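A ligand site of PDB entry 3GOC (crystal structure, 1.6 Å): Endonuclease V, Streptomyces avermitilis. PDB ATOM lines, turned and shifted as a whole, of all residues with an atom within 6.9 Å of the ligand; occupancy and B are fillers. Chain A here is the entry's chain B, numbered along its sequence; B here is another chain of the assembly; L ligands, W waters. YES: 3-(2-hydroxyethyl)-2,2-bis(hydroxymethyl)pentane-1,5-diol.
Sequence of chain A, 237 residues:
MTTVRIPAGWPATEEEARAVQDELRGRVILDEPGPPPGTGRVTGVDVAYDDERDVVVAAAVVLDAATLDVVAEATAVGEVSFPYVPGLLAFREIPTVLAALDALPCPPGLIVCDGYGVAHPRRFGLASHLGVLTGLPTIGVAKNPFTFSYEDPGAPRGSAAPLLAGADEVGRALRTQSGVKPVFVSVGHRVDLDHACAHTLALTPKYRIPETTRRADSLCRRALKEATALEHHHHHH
O9 of the ligand is in hydrogen-bond range of O of Leu 101 (3.2 Å).
O7 of the ligand is in hydrogen-bond range of O of Ala 66 of chain B, 2.7 Å away.
An oxygen (O9) of the ligand lies within hydrogen-bond range of the backbone carbonyl oxygen (O) of Cys 106, at 2.9 Å.
The side-chain carboxylate (OD1) of Asp 102 is in hydrogen-bond range of an oxygen (O4) of the ligand (2.6 Å).
Water W5 bridges O1 of the ligand (2.7 Å) and O of Ala 66 of chain B (2.7 Å).
Water W1 lies within hydrogen-bond range of an oxygen (O3) of the ligand (2.7 Å) and the side-chain carboxylate (OD1) of Asp 102 (2.7 Å).
N of Leu 136 sits close to OG1 of Thr 134 (3.1 Å).
Merely in contact with the ligand: Leu 104 (3.4 Å), Pro 107 (3.6 Å), Pro 108 (3.2 Å), Thr 134 (3.9 Å), Leu 136 (3.7 Å), Thr 67 of chain B (3.9 Å) and Pro 205 of chain B (3.8 Å).
Of the 24 residues printed, 11 come within 4 Å of the ligand.
The nearest printed residue that does not touch the ligand is Leu 68 of chain B (5.1 Å).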
ATOM      1  N   VAL A  62      27.645   2.828  39.691  1.00  0.00           N
ATOM      2  CA  VAL A  62      28.276   4.106  39.984  1.00  0.00           C
ATOM      3  C   VAL A  62      28.507   4.268  41.467  1.00  0.00           C
ATOM      4  O   VAL A  62      27.605   4.087  42.274  1.00  0.00           O
ATOM      5  CB  VAL A  62      27.389   5.280  39.496  1.00  0.00           C
ATOM      6  CG1 VAL A  62      28.132   6.599  39.679  1.00  0.00           C
ATOM      7  CG2 VAL A  62      27.014   5.067  38.045  1.00  0.00           C
ATOM      8  N   LEU A  98      27.215  -0.433  26.602  1.00  0.00           N
ATOM      9  CA  LEU A  98      26.786   0.926  26.344  1.00  0.00           C
ATOM     10  C   LEU A  98      25.318   1.111  26.746  1.00  0.00           C
ATOM     11  O   LEU A  98      24.945   2.168  27.249  1.00  0.00           O
ATOM     12  CB  LEU A  98      26.956   1.270  24.859  1.00  0.00           C
ATOM     13  CG  LEU A  98      28.390   1.418  24.353  1.00  0.00           C
ATOM     14  CD1 LEU A  98      28.375   1.530  22.837  1.00  0.00           C
ATOM     15  CD2 LEU A  98      29.060   2.641  24.977  1.00  0.00           C
ATOM     16  N   ALA A 100      23.778  -0.359  29.173  1.00  0.00           N
ATOM     17  CA  ALA A 100      23.746  -0.248  30.633  1.00  0.00           C
ATOM     18  C   ALA A 100      24.160   1.156  31.045  1.00  0.00           C
ATOM     19  O   ALA A 100      23.518   1.786  31.892  1.00  0.00           O
ATOM     20  CB  ALA A 100      24.669  -1.276  31.278  1.00  0.00           C
ATOM     21  N   LEU A 101      25.234   1.659  30.456  1.00  0.00           N
ATOM     22  CA  LEU A 101      25.710   3.006  30.768  1.00  0.00           C
ATOM     23  C   LEU A 101      24.640   4.038  30.406  1.00  0.00           C
ATOM     24  O   LEU A 101      24.393   4.958  31.177  1.00  0.00           O
ATOM     25  CB  LEU A 101      27.001   3.300  30.007  1.00  0.00           C
ATOM     26  CG  LEU A 101      28.224   2.500  30.484  1.00  0.00           C
ATOM     27  CD1 LEU A 101      29.353   2.653  29.475  1.00  0.00           C
ATOM     28  CD2 LEU A 101      28.673   2.993  31.866  1.00  0.00           C
ATOM     29  N   ASP A 102      24.011   3.875  29.247  1.00  0.00           N
ATOM     30  CA  ASP A 102      22.981   4.808  28.814  1.00  0.00           C
ATOM     31  C   ASP A 102      21.804   4.888  29.780  1.00  0.00           C
ATOM     32  O   ASP A 102      21.161   5.922  29.905  1.00  0.00           O
ATOM     33  CB  ASP A 102      22.436   4.432  27.428  1.00  0.00           C
ATOM     34  CG  ASP A 102      23.423   4.689  26.309  1.00  0.00           C
ATOM     35  OD1 ASP A 102      24.480   5.300  26.564  1.00  0.00           O
ATOM     36  OD2 ASP A 102      23.147   4.276  25.164  1.00  0.00           O
ATOM     37  N   ALA A 103      21.530   3.771  30.457  1.00  0.00           N
ATOM     38  CA  ALA A 103      20.414   3.687  31.399  1.00  0.00           C
ATOM     39  C   ALA A 103      20.687   4.305  32.768  1.00  0.00           C
ATOM     40  O   ALA A 103      19.805   4.353  33.620  1.00  0.00           O
ATOM     41  CB  ALA A 103      19.981   2.233  31.562  1.00  0.00           C
ATOM     42  N   LEU A 104      21.919   4.758  32.988  1.00  0.00           N
ATOM     43  CA  LEU A 104      22.290   5.365  34.255  1.00  0.00           C
ATOM     44  C   LEU A 104      21.657   6.747  34.412  1.00  0.00           C
ATOM     45  O   LEU A 104      21.465   7.471  33.431  1.00  0.00           O
ATOM     46  CB  LEU A 104      23.811   5.501  34.370  1.00  0.00           C
ATOM     47  CG  LEU A 104      24.591   4.204  34.584  1.00  0.00           C
ATOM     48  CD1 LEU A 104      26.085   4.501  34.569  1.00  0.00           C
ATOM     49  CD2 LEU A 104      24.191   3.572  35.911  1.00  0.00           C
ATOM     50  N   PRO A 105      21.318   7.132  35.646  1.00  0.00           N
ATOM     51  CA  PRO A 105      20.701   8.423  35.942  1.00  0.00           C
ATOM     52  C   PRO A 105      21.698   9.578  36.117  1.00  0.00           C
ATOM     53  O   PRO A 105      21.293  10.716  36.359  1.00  0.00           O
ATOM     54  CB  PRO A 105      19.926   8.147  37.213  1.00  0.00           C
ATOM     55  CG  PRO A 105      20.859   7.226  37.939  1.00  0.00           C
ATOM     56  CD  PRO A 105      21.309   6.269  36.853  1.00  0.00           C
ATOM     57  N   CYS A 106      22.981   9.270  36.003  1.00  0.00           N
ATOM     58  CA  CYS A 106      24.029  10.280  36.187  1.00  0.00           C
ATOM     59  C   CYS A 106      25.260   9.962  35.342  1.00  0.00           C
ATOM     60  O   CYS A 106      25.427   8.845  34.861  1.00  0.00           O
ATOM     61  CB  CYS A 106      24.436  10.327  37.655  1.00  0.00           C
ATOM     62  SG  CYS A 106      25.137   8.747  38.270  1.00  0.00           S
ATOM     63  N   PRO A 107      26.145  10.956  35.144  1.00  0.00           N
ATOM     64  CA  PRO A 107      27.360  10.730  34.351  1.00  0.00           C
ATOM     65  C   PRO A 107      28.246   9.733  35.092  1.00  0.00           C
ATOM     66  O   PRO A 107      28.348   9.769  36.321  1.00  0.00           O
ATOM     67  CB  PRO A 107      27.993  12.119  34.277  1.00  0.00           C
ATOM     68  CG  PRO A 107      26.801  13.049  34.391  1.00  0.00           C
ATOM     69  CD  PRO A 107      25.991  12.391  35.481  1.00  0.00           C
ATOM     70  N   PRO A 108      28.913   8.819  34.360  1.00  0.00           N
ATOM     71  CA  PRO A 108      29.794   7.802  34.961  1.00  0.00           C
ATOM     72  C   PRO A 108      31.017   8.335  35.694  1.00  0.00           C
ATOM     73  O   PRO A 108      31.465   7.720  36.667  1.00  0.00           O
ATOM     74  CB  PRO A 108      30.191   6.932  33.769  1.00  0.00           C
ATOM     75  CG  PRO A 108      29.046   7.097  32.811  1.00  0.00           C
ATOM     76  CD  PRO A 108      28.738   8.566  32.913  1.00  0.00           C
ATOM     77  N   GLY A 109      31.563   9.454  35.220  1.00  0.00           N
ATOM     78  CA  GLY A 109      32.741  10.034  35.850  1.00  0.00           C
ATOM     79  C   GLY A 109      34.038   9.450  35.312  1.00  0.00           C
ATOM     80  O   GLY A 109      34.780  10.097  34.574  1.00  0.00           O
ATOM     81  N   ILE A 111      35.224   5.373  34.072  1.00  0.00           N
ATOM     82  CA  ILE A 111      34.814   3.975  33.914  1.00  0.00           C
ATOM     83  C   ILE A 111      35.983   3.022  34.169  1.00  0.00           C
ATOM     84  O   ILE A 111      37.021   3.122  33.514  1.00  0.00           O
ATOM     85  CB  ILE A 111      34.261   3.707  32.501  1.00  0.00           C
ATOM     86  CG1 ILE A 111      33.057   4.613  32.233  1.00  0.00           C
ATOM     87  CG2 ILE A 111      33.859   2.251  32.375  1.00  0.00           C
ATOM     88  CD1 ILE A 111      32.484   4.465  30.841  1.00  0.00           C
ATOM     89  N   THR A 134      32.506   6.597  24.084  1.00  0.00           N
ATOM     90  CA  THR A 134      31.765   7.431  25.022  1.00  0.00           C
ATOM     91  C   THR A 134      32.429   8.774  25.300  1.00  0.00           C
ATOM     92  O   THR A 134      31.790   9.689  25.813  1.00  0.00           O
ATOM     93  CB  THR A 134      31.612   6.726  26.370  1.00  0.00           C
ATOM     94  OG1 THR A 134      32.912   6.563  26.952  1.00  0.00           O
ATOM     95  CG2 THR A 134      30.968   5.362  26.201  1.00  0.00           C
ATOM     96  N   LEU A 136      34.463   9.242  27.510  1.00  0.00           N
ATOM     97  CA  LEU A 136      34.751   9.279  28.952  1.00  0.00           C
ATOM     98  C   LEU A 136      36.126   8.720  29.338  1.00  0.00           C
ATOM     99  O   LEU A 136      36.724   7.936  28.589  1.00  0.00           O
ATOM    100  CB  LEU A 136      33.674   8.480  29.699  1.00  0.00           C
ATOM    101  CG  LEU A 136      32.216   8.944  29.641  1.00  0.00           C
ATOM    102  CD1 LEU A 136      31.319   7.788  30.059  1.00  0.00           C
ATOM    103  CD2 LEU A 136      32.007  10.141  30.555  1.00  0.00           C
ATOM    104  N   GLY B  38      32.025  16.039  27.592  1.00  0.00           N
ATOM    105  CA  GLY B  38      31.523  15.613  28.890  1.00  0.00           C
ATOM    106  C   GLY B  38      31.829  16.470  30.099  1.00  0.00           C
ATOM    107  O   GLY B  38      31.583  16.043  31.230  1.00  0.00           O
ATOM    108  N   ALA B  65      27.568  19.846  29.592  1.00  0.00           N
ATOM    109  CA  ALA B  65      28.152  18.802  28.757  1.00  0.00           C
ATOM    110  C   ALA B  65      28.090  17.398  29.338  1.00  0.00           C
ATOM    111  O   ALA B  65      27.916  16.417  28.609  1.00  0.00           O
ATOM    112  CB  ALA B  65      29.590  19.163  28.425  1.00  0.00           C
ATOM    113  N   ALA B  66      28.225  17.292  30.660  1.00  0.00           N
ATOM    114  CA  ALA B  66      28.211  15.980  31.301  1.00  0.00           C
ATOM    115  C   ALA B  66      26.852  15.285  31.258  1.00  0.00           C
ATOM    116  O   ALA B  66      26.782  14.075  31.027  1.00  0.00           O
ATOM    117  CB  ALA B  66      28.677  16.115  32.739  1.00  0.00           C
ATOM    118  N   THR B  67      25.782  16.048  31.484  1.00  0.00           N
ATOM    119  CA  THR B  67      24.428  15.489  31.519  1.00  0.00           C
ATOM    120  C   THR B  67      23.589  15.776  30.285  1.00  0.00           C
ATOM    121  O   THR B  67      22.612  15.074  30.003  1.00  0.00           O
ATOM    122  CB  THR B  67      23.655  16.050  32.719  1.00  0.00           C
ATOM    123  OG1 THR B  67      23.535  17.471  32.562  1.00  0.00           O
ATOM    124  CG2 THR B  67      24.385  15.760  34.012  1.00  0.00           C
ATOM    125  N   LEU B  68      23.970  16.815  29.553  1.00  0.00           N
ATOM    126  CA  LEU B  68      23.266  17.287  28.364  1.00  0.00           C
ATOM    127  C   LEU B  68      22.004  18.050  28.753  1.00  0.00           C
ATOM    128  O   LEU B  68      21.168  18.370  27.907  1.00  0.00           O
ATOM    129  CB  LEU B  68      22.925  16.136  27.410  1.00  0.00           C
ATOM    130  CG  LEU B  68      24.106  15.397  26.776  1.00  0.00           C
ATOM    131  CD1 LEU B  68      23.606  14.477  25.675  1.00  0.00           C
ATOM    132  CD2 LEU B  68      25.105  16.386  26.201  1.00  0.00           C
ATOM    133  N   ARG B 157      28.730   3.216  14.863  1.00  0.00           N
ATOM    134  CA  ARG B 157      28.768   4.570  15.397  1.00  0.00           C
ATOM    135  C   ARG B 157      30.206   4.854  15.819  1.00  0.00           C
ATOM    136  O   ARG B 157      30.879   3.985  16.375  1.00  0.00           O
ATOM    137  CB  ARG B 157      27.830   4.671  16.606  1.00  0.00           C
ATOM    138  CG  ARG B 157      28.048   5.883  17.537  1.00  0.00           C
ATOM    139  CD  ARG B 157      26.933   5.957  18.584  1.00  0.00           C
ATOM    140  NE  ARG B 157      27.285   6.699  19.801  1.00  0.00           N
ATOM    141  CZ  ARG B 157      27.299   8.025  19.910  1.00  0.00           C
ATOM    142  NH1 ARG B 157      27.630   8.588  21.071  1.00  0.00           N
ATOM    143  NH2 ARG B 157      26.981   8.787  18.872  1.00  0.00           N
ATOM    144  N   ALA B 202      29.536  12.763  21.667  1.00  0.00           N
ATOM    145  CA  ALA B 202      29.016  12.954  23.009  1.00  0.00           C
ATOM    146  C   ALA B 202      27.651  13.638  23.001  1.00  0.00           C
ATOM    147  O   ALA B 202      26.890  13.528  23.966  1.00  0.00           O
ATOM    148  CB  ALA B 202      30.002  13.751  23.854  1.00  0.00           C
ATOM    149  N   PRO B 205      24.266  10.535  21.698  1.00  0.00           N
ATOM    150  CA  PRO B 205      24.088   9.159  22.187  1.00  0.00           C
ATOM    151  C   PRO B 205      22.742   8.556  21.785  1.00  0.00           C
ATOM    152  O   PRO B 205      22.619   7.335  21.659  1.00  0.00           O
ATOM    153  CB  PRO B 205      24.226   9.319  23.701  1.00  0.00           C
ATOM    154  CG  PRO B 205      23.617  10.659  23.939  1.00  0.00           C
ATOM    155  CD  PRO B 205      24.237  11.488  22.824  1.00  0.00           C
ATOM    156  N   LYS B 206      21.751   9.416  21.563  1.00  0.00           N
ATOM    157  CA  LYS B 206      20.400   8.969  21.231  1.00  0.00           C
ATOM    158  C   LYS B 206      19.955   9.253  19.801  1.00  0.00           C
ATOM    159  O   LYS B 206      19.270   8.445  19.190  1.00  0.00           O
ATOM    160  CB  LYS B 206      19.396   9.601  22.190  1.00  0.00           C
ATOM    161  CG  LYS B 206      19.730   9.424  23.659  1.00  0.00           C
ATOM    162  CD  LYS B 206      18.793  10.244  24.533  1.00  0.00           C
ATOM    163  CE  LYS B 206      19.201  10.189  25.992  1.00  0.00           C
ATOM    164  NZ  LYS B 206      18.299  11.023  26.846  1.00  0.00           N
HETATM  165  O1  YES L   1      28.275   9.933  30.108  1.00  0.00           O
HETATM  166  C1  YES L   1      27.712   9.583  28.883  1.00  0.00           C
HETATM  167  C2  YES L   1      26.571   8.704  28.759  1.00  0.00           C
HETATM  168  C3  YES L   1      27.028   7.326  29.311  1.00  0.00           C
HETATM  169  O3  YES L   1      28.141   6.682  28.570  1.00  0.00           O
HETATM  170  C4  YES L   1      26.069   8.714  27.298  1.00  0.00           C
HETATM  171  O4  YES L   1      24.845   7.778  27.110  1.00  0.00           O
HETATM  172  C5  YES L   1      25.432   9.384  29.667  1.00  0.00           C
HETATM  173  C6  YES L   1      24.862  10.787  29.159  1.00  0.00           C
HETATM  174  C7  YES L   1      24.481  11.706  30.272  1.00  0.00           C
HETATM  175  O7  YES L   1      25.441  11.741  31.317  1.00  0.00           O
HETATM  176  C8  YES L   1      24.177   8.492  29.979  1.00  0.00           C
HETATM  177  C9  YES L   1      24.123   8.285  31.426  1.00  0.00           C
HETATM  178  O9  YES L   1      25.238   7.890  32.181  1.00  0.00           O
HETATM  179  O   HOH W   1      27.184   4.933  26.791  1.00  0.00           O
HETATM  180  O   HOH W   2      22.325   8.900  26.689  1.00  0.00           O
HETATM  181  O   HOH W   3      23.232  12.010  33.342  1.00  0.00           O
HETATM  182  O   HOH W   4      22.010  11.538  27.567  1.00  0.00           O
HETATM  183  O   HOH W   5      28.848  12.541  30.082  1.00  0.00           O
